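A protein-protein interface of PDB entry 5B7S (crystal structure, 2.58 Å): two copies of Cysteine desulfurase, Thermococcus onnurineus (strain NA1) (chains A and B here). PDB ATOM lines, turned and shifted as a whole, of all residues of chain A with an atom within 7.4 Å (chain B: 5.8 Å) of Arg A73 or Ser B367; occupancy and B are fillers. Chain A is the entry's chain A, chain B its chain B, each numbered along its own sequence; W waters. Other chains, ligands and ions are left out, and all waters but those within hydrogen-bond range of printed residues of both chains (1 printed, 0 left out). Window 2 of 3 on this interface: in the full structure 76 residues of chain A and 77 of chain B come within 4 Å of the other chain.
The backbone NH of Arg A73 is in hydrogen-bond range of the side-chain carboxylate of Asp B364, 3.0 Å away. The side-chain hydroxyl of Ser B367 lies within hydrogen-bond range of the guanidinium group of Arg A73 (3.1 Å).
The backbone NH (N) of Ser A75 sits at hydrogen-bond distance from a ring nitrogen (ND1) of His A72, at 3.3 Å. N of Ile B38 lies within hydrogen-bond range of O of Ser B367 (3.0 Å). O of Ile B38 is in hydrogen-bond range of N of Met B369 (2.8 Å).
His A72 touches Asp B364. His A72 touches Met B369 (CB to SD, 3.6 Å). Arg A73 touches Val B37 (NH2 to CG1, 3.9 Å). Leu A74 touches Tyr B39 (CD2 to CD1, 3.99 Å).
Ser B367 touches one residue of chain A. Of the printed residues of chain B, His A72 touches Asp B364 (3.5 Å) and Met B369 (3.6 Å). Of the printed residues of chain A, Met B369 touches His A72. The nearest residue of chain B that does not touch Arg A73 is Met B369 (4.04 Å). The nearest printed residue of chain A that does not touch Ser B367 is His A72 (7.5 Å). The nearest printed residue of chain A that does not touch Met B369 is Arg A73 (4.04 Å).
Hydrophobic or aromatic side chains of chain A that line the printed part of chain B: His A72 and Leu A74. Printed residues of chain B that touch a printed residue of chain A: Val B37, Tyr B39, Asp B364, Ser B367 and Met B369. Along chain B the printed residues that touch a printed residue of chain A span positions 37 to 369. Among the printed residues, 6 pairs touch across the chains.
No position is printed for both chains.
Water W1 lies within hydrogen-bond range of O of Val A71 (2.7 Å) and OD2 of Asp B364 (2.9 Å).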
ATOM      1  N   TYR A  63       3.603 -15.556  32.039  1.00  0.00           N
ATOM      2  CA  TYR A  63       4.702 -16.250  31.381  1.00  0.00           C
ATOM      3  C   TYR A  63       5.488 -17.181  32.306  1.00  0.00           C
ATOM      4  O   TYR A  63       6.707 -17.343  32.188  1.00  0.00           O
ATOM      5  CB  TYR A  63       5.579 -15.267  30.625  1.00  0.00           C
ATOM      6  CG  TYR A  63       6.206 -14.172  31.458  1.00  0.00           C
ATOM      7  CD1 TYR A  63       5.541 -12.959  31.680  1.00  0.00           C
ATOM      8  CD2 TYR A  63       7.479 -14.308  31.971  1.00  0.00           C
ATOM      9  CE1 TYR A  63       6.126 -11.943  32.427  1.00  0.00           C
ATOM     10  CE2 TYR A  63       8.070 -13.289  32.704  1.00  0.00           C
ATOM     11  CZ  TYR A  63       7.391 -12.120  32.922  1.00  0.00           C
ATOM     12  OH  TYR A  63       7.985 -11.152  33.647  1.00  0.00           O
ATOM     13  N   ALA A  65       7.329 -20.198  33.847  1.00  0.00           N
ATOM     14  CA  ALA A  65       8.220 -21.225  33.264  1.00  0.00           C
ATOM     15  C   ALA A  65       9.608 -21.151  33.924  1.00  0.00           C
ATOM     16  O   ALA A  65       9.886 -20.166  34.592  1.00  0.00           O
ATOM     17  CB  ALA A  65       8.333 -21.044  31.769  1.00  0.00           C
ATOM     18  N   GLY A  70      15.113 -22.805  27.280  1.00  0.00           N
ATOM     19  CA  GLY A  70      14.246 -23.893  26.779  1.00  0.00           C
ATOM     20  C   GLY A  70      13.432 -23.383  25.605  1.00  0.00           C
ATOM     21  O   GLY A  70      13.086 -22.193  25.564  1.00  0.00           O
ATOM     22  N   VAL A  71      13.132 -24.266  24.661  1.00  0.00           N
ATOM     23  CA  VAL A  71      12.661 -23.864  23.332  1.00  0.00           C
ATOM     24  C   VAL A  71      11.278 -23.258  23.303  1.00  0.00           C
ATOM     25  O   VAL A  71      10.986 -22.457  22.427  1.00  0.00           O
ATOM     26  CB  VAL A  71      12.746 -25.057  22.337  1.00  0.00           C
ATOM     27  CG1 VAL A  71      11.994 -24.820  21.041  1.00  0.00           C
ATOM     28  CG2 VAL A  71      14.197 -25.359  22.027  1.00  0.00           C
ATOM     29  N   HIS A  72      10.416 -23.633  24.242  1.00  0.00           N
ATOM     30  CA  HIS A  72       9.051 -23.136  24.193  1.00  0.00           C
ATOM     31  C   HIS A  72       8.966 -21.636  24.557  1.00  0.00           C
ATOM     32  O   HIS A  72       9.898 -21.068  25.140  1.00  0.00           O
ATOM     33  CB  HIS A  72       8.075 -24.073  24.927  1.00  0.00           C
ATOM     34  CG  HIS A  72       8.242 -24.147  26.409  1.00  0.00           C
ATOM     35  ND1 HIS A  72       7.933 -23.098  27.248  1.00  0.00           N
ATOM     36  CD2 HIS A  72       8.591 -25.176  27.212  1.00  0.00           C
ATOM     37  CE1 HIS A  72       8.127 -23.468  28.500  1.00  0.00           C
ATOM     38  NE2 HIS A  72       8.538 -24.720  28.505  1.00  0.00           N
ATOM     39  N   ARG A  73       7.901 -20.970  24.109  1.00  0.00           N
ATOM     40  CA  ARG A  73       7.876 -19.498  24.168  1.00  0.00           C
ATOM     41  C   ARG A  73       7.766 -18.887  25.571  1.00  0.00           C
ATOM     42  O   ARG A  73       8.125 -17.728  25.767  1.00  0.00           O
ATOM     43  CB  ARG A  73       6.802 -18.909  23.258  1.00  0.00           C
ATOM     44  CG  ARG A  73       5.395 -19.392  23.513  1.00  0.00           C
ATOM     45  CD  ARG A  73       4.393 -18.333  23.107  1.00  0.00           C
ATOM     46  NE  ARG A  73       3.050 -18.890  22.960  1.00  0.00           N
ATOM     47  CZ  ARG A  73       2.624 -19.611  21.923  1.00  0.00           C
ATOM     48  NH1 ARG A  73       3.435 -19.903  20.900  1.00  0.00           N
ATOM     49  NH2 ARG A  73       1.361 -20.057  21.920  1.00  0.00           N
ATOM     50  N   LEU A  74       7.245 -19.656  26.512  1.00  0.00           N
ATOM     51  CA  LEU A  74       7.195 -19.276  27.923  1.00  0.00           C
ATOM     52  C   LEU A  74       8.581 -19.284  28.576  1.00  0.00           C
ATOM     53  O   LEU A  74       8.959 -18.337  29.261  1.00  0.00           O
ATOM     54  CB  LEU A  74       6.215 -20.186  28.698  1.00  0.00           C
ATOM     55  CG  LEU A  74       4.758 -19.731  28.833  1.00  0.00           C
ATOM     56  CD1 LEU A  74       4.209 -18.978  27.629  1.00  0.00           C
ATOM     57  CD2 LEU A  74       3.873 -20.926  29.165  1.00  0.00           C
ATOM     58  N   SER A  75       9.334 -20.336  28.349  1.00  0.00           N
ATOM     59  CA  SER A  75      10.704 -20.423  28.804  1.00  0.00           C
ATOM     60  C   SER A  75      11.573 -19.386  28.097  1.00  0.00           C
ATOM     61  O   SER A  75      12.477 -18.844  28.730  1.00  0.00           O
ATOM     62  CB  SER A  75      11.271 -21.846  28.607  1.00  0.00           C
ATOM     63  OG  SER A  75      12.535 -22.041  29.244  1.00  0.00           O
ATOM     64  N   GLN A  76      11.291 -19.116  26.816  1.00  0.00           N
ATOM     65  CA  GLN A  76      11.927 -18.023  26.083  1.00  0.00           C
ATOM     66  C   GLN A  76      11.677 -16.740  26.799  1.00  0.00           C
ATOM     67  O   GLN A  76      12.630 -16.024  27.135  1.00  0.00           O
ATOM     68  CB  GLN A  76      11.397 -17.854  24.641  1.00  0.00           C
ATOM     69  CG  GLN A  76      11.950 -18.828  23.610  1.00  0.00           C
ATOM     70  CD  GLN A  76      13.447 -18.632  23.303  1.00  0.00           C
ATOM     71  OE1 GLN A  76      13.854 -17.600  22.728  1.00  0.00           O
ATOM     72  NE2 GLN A  76      14.276 -19.641  23.669  1.00  0.00           N
ATOM     73  N   MET A  77      10.403 -16.438  27.020  1.00  0.00           N
ATOM     74  CA  MET A  77      10.041 -15.189  27.714  1.00  0.00           C
ATOM     75  C   MET A  77      10.644 -15.096  29.130  1.00  0.00           C
ATOM     76  O   MET A  77      11.258 -14.099  29.484  1.00  0.00           O
ATOM     77  CB  MET A  77       8.523 -14.988  27.785  1.00  0.00           C
ATOM     78  CG  MET A  77       8.101 -13.706  28.529  1.00  0.00           C
ATOM     79  SD  MET A  77       8.313 -12.104  27.675  1.00  0.00           S
ATOM     80  CE  MET A  77      10.062 -11.773  27.605  1.00  0.00           C
ATOM     81  N   ALA A  78      10.475 -16.149  29.916  1.00  0.00           N
ATOM     82  CA  ALA A  78      10.942 -16.149  31.271  1.00  0.00           C
ATOM     83  C   ALA A  78      12.456 -15.967  31.311  1.00  0.00           C
ATOM     84  O   ALA A  78      12.984 -15.214  32.131  1.00  0.00           O
ATOM     85  CB  ALA A  78      10.502 -17.436  31.970  1.00  0.00           C
ATOM     86  N   THR A  79      13.150 -16.644  30.417  1.00  0.00           N
ATOM     87  CA  THR A  79      14.609 -16.588  30.379  1.00  0.00           C
ATOM     88  C   THR A  79      15.044 -15.201  30.030  1.00  0.00           C
ATOM     89  O   THR A  79      15.903 -14.643  30.710  1.00  0.00           O
ATOM     90  CB  THR A  79      15.223 -17.569  29.340  1.00  0.00           C
ATOM     91  OG1 THR A  79      14.919 -18.926  29.698  1.00  0.00           O
ATOM     92  CG2 THR A  79      16.706 -17.449  29.286  1.00  0.00           C
ATOM     93  N   GLU B  36      -4.448 -20.375  27.012  1.00  0.00           N
ATOM     94  CA  GLU B  36      -3.490 -19.759  26.097  1.00  0.00           C
ATOM     95  C   GLU B  36      -2.565 -20.778  25.441  1.00  0.00           C
ATOM     96  O   GLU B  36      -2.170 -20.615  24.272  1.00  0.00           O
ATOM     97  CB  GLU B  36      -2.631 -18.751  26.876  1.00  0.00           C
ATOM     98  CG  GLU B  36      -3.376 -17.540  27.431  1.00  0.00           C
ATOM     99  CD  GLU B  36      -4.352 -16.951  26.418  1.00  0.00           C
ATOM    100  OE1 GLU B  36      -5.573 -17.221  26.537  1.00  0.00           O
ATOM    101  OE2 GLU B  36      -3.893 -16.274  25.473  1.00  0.00           O
ATOM    102  N   VAL B  37      -2.179 -21.790  26.226  1.00  0.00           N
ATOM    103  CA  VAL B  37      -1.297 -22.861  25.800  1.00  0.00           C
ATOM    104  C   VAL B  37      -1.617 -24.195  26.515  1.00  0.00           C
ATOM    105  O   VAL B  37      -2.209 -24.227  27.578  1.00  0.00           O
ATOM    106  CB  VAL B  37       0.174 -22.521  26.126  1.00  0.00           C
ATOM    107  CG1 VAL B  37       0.585 -21.165  25.559  1.00  0.00           C
ATOM    108  CG2 VAL B  37       0.444 -22.569  27.620  1.00  0.00           C
ATOM    109  N   ILE B  38      -1.129 -25.269  25.925  1.00  0.00           N
ATOM    110  CA  ILE B  38      -1.108 -26.591  26.502  1.00  0.00           C
ATOM    111  C   ILE B  38       0.253 -26.779  27.180  1.00  0.00           C
ATOM    112  O   ILE B  38       1.292 -26.960  26.519  1.00  0.00           O
ATOM    113  CB  ILE B  38      -1.273 -27.633  25.401  1.00  0.00           C
ATOM    114  CG1 ILE B  38      -2.548 -27.307  24.576  1.00  0.00           C
ATOM    115  CG2 ILE B  38      -1.253 -29.038  26.023  1.00  0.00           C
ATOM    116  CD1 ILE B  38      -2.967 -28.324  23.529  1.00  0.00           C
ATOM    117  N   TYR B  39       0.244 -26.720  28.505  1.00  0.00           N
ATOM    118  CA  TYR B  39       1.479 -26.680  29.261  1.00  0.00           C
ATOM    119  C   TYR B  39       1.816 -28.098  29.731  1.00  0.00           C
ATOM    120  O   TYR B  39       1.272 -28.576  30.716  1.00  0.00           O
ATOM    121  CB  TYR B  39       1.349 -25.708  30.442  1.00  0.00           C
ATOM    122  CG  TYR B  39       2.635 -25.503  31.201  1.00  0.00           C
ATOM    123  CD1 TYR B  39       3.542 -24.555  30.798  1.00  0.00           C
ATOM    124  CD2 TYR B  39       2.951 -26.282  32.317  1.00  0.00           C
ATOM    125  CE1 TYR B  39       4.729 -24.356  31.486  1.00  0.00           C
ATOM    126  CE2 TYR B  39       4.141 -26.099  33.011  1.00  0.00           C
ATOM    127  CZ  TYR B  39       5.030 -25.132  32.582  1.00  0.00           C
ATOM    128  OH  TYR B  39       6.204 -24.897  33.242  1.00  0.00           O
ATOM    129  N   LEU B 363       6.120 -28.516  18.279  1.00  0.00           N
ATOM    130  CA  LEU B 363       5.018 -28.479  19.263  1.00  0.00           C
ATOM    131  C   LEU B 363       4.666 -27.043  19.766  1.00  0.00           C
ATOM    132  O   LEU B 363       3.483 -26.671  19.873  1.00  0.00           O
ATOM    133  CB  LEU B 363       5.352 -29.360  20.490  1.00  0.00           C
ATOM    134  CG  LEU B 363       5.121 -30.873  20.570  1.00  0.00           C
ATOM    135  CD1 LEU B 363       4.073 -31.316  19.587  1.00  0.00           C
ATOM    136  CD2 LEU B 363       6.368 -31.686  20.396  1.00  0.00           C
ATOM    137  N   ASP B 364       5.703 -26.267  20.082  1.00  0.00           N
ATOM    138  CA  ASP B 364       5.566 -24.844  20.390  1.00  0.00           C
ATOM    139  C   ASP B 364       4.851 -24.051  19.286  1.00  0.00           C
ATOM    140  O   ASP B 364       4.050 -23.163  19.603  1.00  0.00           O
ATOM    141  CB  ASP B 364       6.938 -24.228  20.662  1.00  0.00           C
ATOM    142  CG  ASP B 364       6.853 -22.779  21.077  1.00  0.00           C
ATOM    143  OD1 ASP B 364       6.284 -22.506  22.163  1.00  0.00           O
ATOM    144  OD2 ASP B 364       7.366 -21.908  20.314  1.00  0.00           O
ATOM    145  N   ASP B 365       5.106 -24.360  18.012  1.00  0.00           N
ATOM    146  CA  ASP B 365       4.344 -23.714  16.930  1.00  0.00           C
ATOM    147  C   ASP B 365       2.823 -23.973  17.055  1.00  0.00           C
ATOM    148  O   ASP B 365       2.022 -23.129  16.682  1.00  0.00           O
ATOM    149  CB  ASP B 365       4.848 -24.147  15.539  1.00  0.00           C
ATOM    150  CG  ASP B 365       6.169 -23.530  15.175  1.00  0.00           C
ATOM    151  OD1 ASP B 365       6.476 -22.426  15.665  1.00  0.00           O
ATOM    152  OD2 ASP B 365       6.912 -24.156  14.396  1.00  0.00           O
ATOM    153  N   HIS B 366       2.453 -25.134  17.597  1.00  0.00           N
ATOM    154  CA  HIS B 366       1.076 -25.489  17.890  1.00  0.00           C
ATOM    155  C   HIS B 366       0.635 -25.161  19.337  1.00  0.00           C
ATOM    156  O   HIS B 366      -0.315 -25.768  19.880  1.00  0.00           O
ATOM    157  CB  HIS B 366       0.904 -26.982  17.547  1.00  0.00           C
ATOM    158  CG  HIS B 366       0.936 -27.255  16.069  1.00  0.00           C
ATOM    159  ND1 HIS B 366       2.086 -27.597  15.397  1.00  0.00           N
ATOM    160  CD2 HIS B 366      -0.032 -27.175  15.127  1.00  0.00           C
ATOM    161  CE1 HIS B 366       1.819 -27.764  14.116  1.00  0.00           C
ATOM    162  NE2 HIS B 366       0.541 -27.508  13.925  1.00  0.00           N
ATOM    163  N   SER B 367       1.325 -24.204  19.960  1.00  0.00           N
ATOM    164  CA  SER B 367       1.051 -23.782  21.324  1.00  0.00           C
ATOM    165  C   SER B 367       1.096 -24.903  22.370  1.00  0.00           C
ATOM    166  O   SER B 367       0.421 -24.796  23.397  1.00  0.00           O
ATOM    167  CB  SER B 367      -0.315 -23.076  21.391  1.00  0.00           C
ATOM    168  OG  SER B 367      -0.431 -22.075  20.414  1.00  0.00           O
ATOM    169  N   ILE B 368       1.884 -25.957  22.129  1.00  0.00           N
ATOM    170  CA  ILE B 368       2.100 -27.028  23.107  1.00  0.00           C
ATOM    171  C   ILE B 368       3.518 -26.939  23.677  1.00  0.00           C
ATOM    172  O   ILE B 368       4.475 -27.086  22.936  1.00  0.00           O
ATOM    173  CB  ILE B 368       1.940 -28.399  22.474  1.00  0.00           C
ATOM    174  CG1 ILE B 368       0.498 -28.593  22.032  1.00  0.00           C
ATOM    175  CG2 ILE B 368       2.329 -29.487  23.484  1.00  0.00           C
ATOM    176  CD1 ILE B 368       0.290 -29.758  21.072  1.00  0.00           C
ATOM    177  N   MET B 369       3.630 -26.756  24.997  1.00  0.00           N
ATOM    178  CA  MET B 369       4.904 -26.497  25.668  1.00  0.00           C
ATOM    179  C   MET B 369       5.478 -27.783  26.267  1.00  0.00           C
ATOM    180  O   MET B 369       4.865 -28.401  27.100  1.00  0.00           O
ATOM    181  CB  MET B 369       4.762 -25.458  26.786  1.00  0.00           C
ATOM    182  CG  MET B 369       3.935 -24.205  26.485  1.00  0.00           C
ATOM    183  SD  MET B 369       4.628 -22.985  25.344  1.00  0.00           S
ATOM    184  CE  MET B 369       3.530 -23.166  23.939  1.00  0.00           C
HETATM  185  O   HOH W   1       9.809 -20.448  21.043  1.00  0.00           O
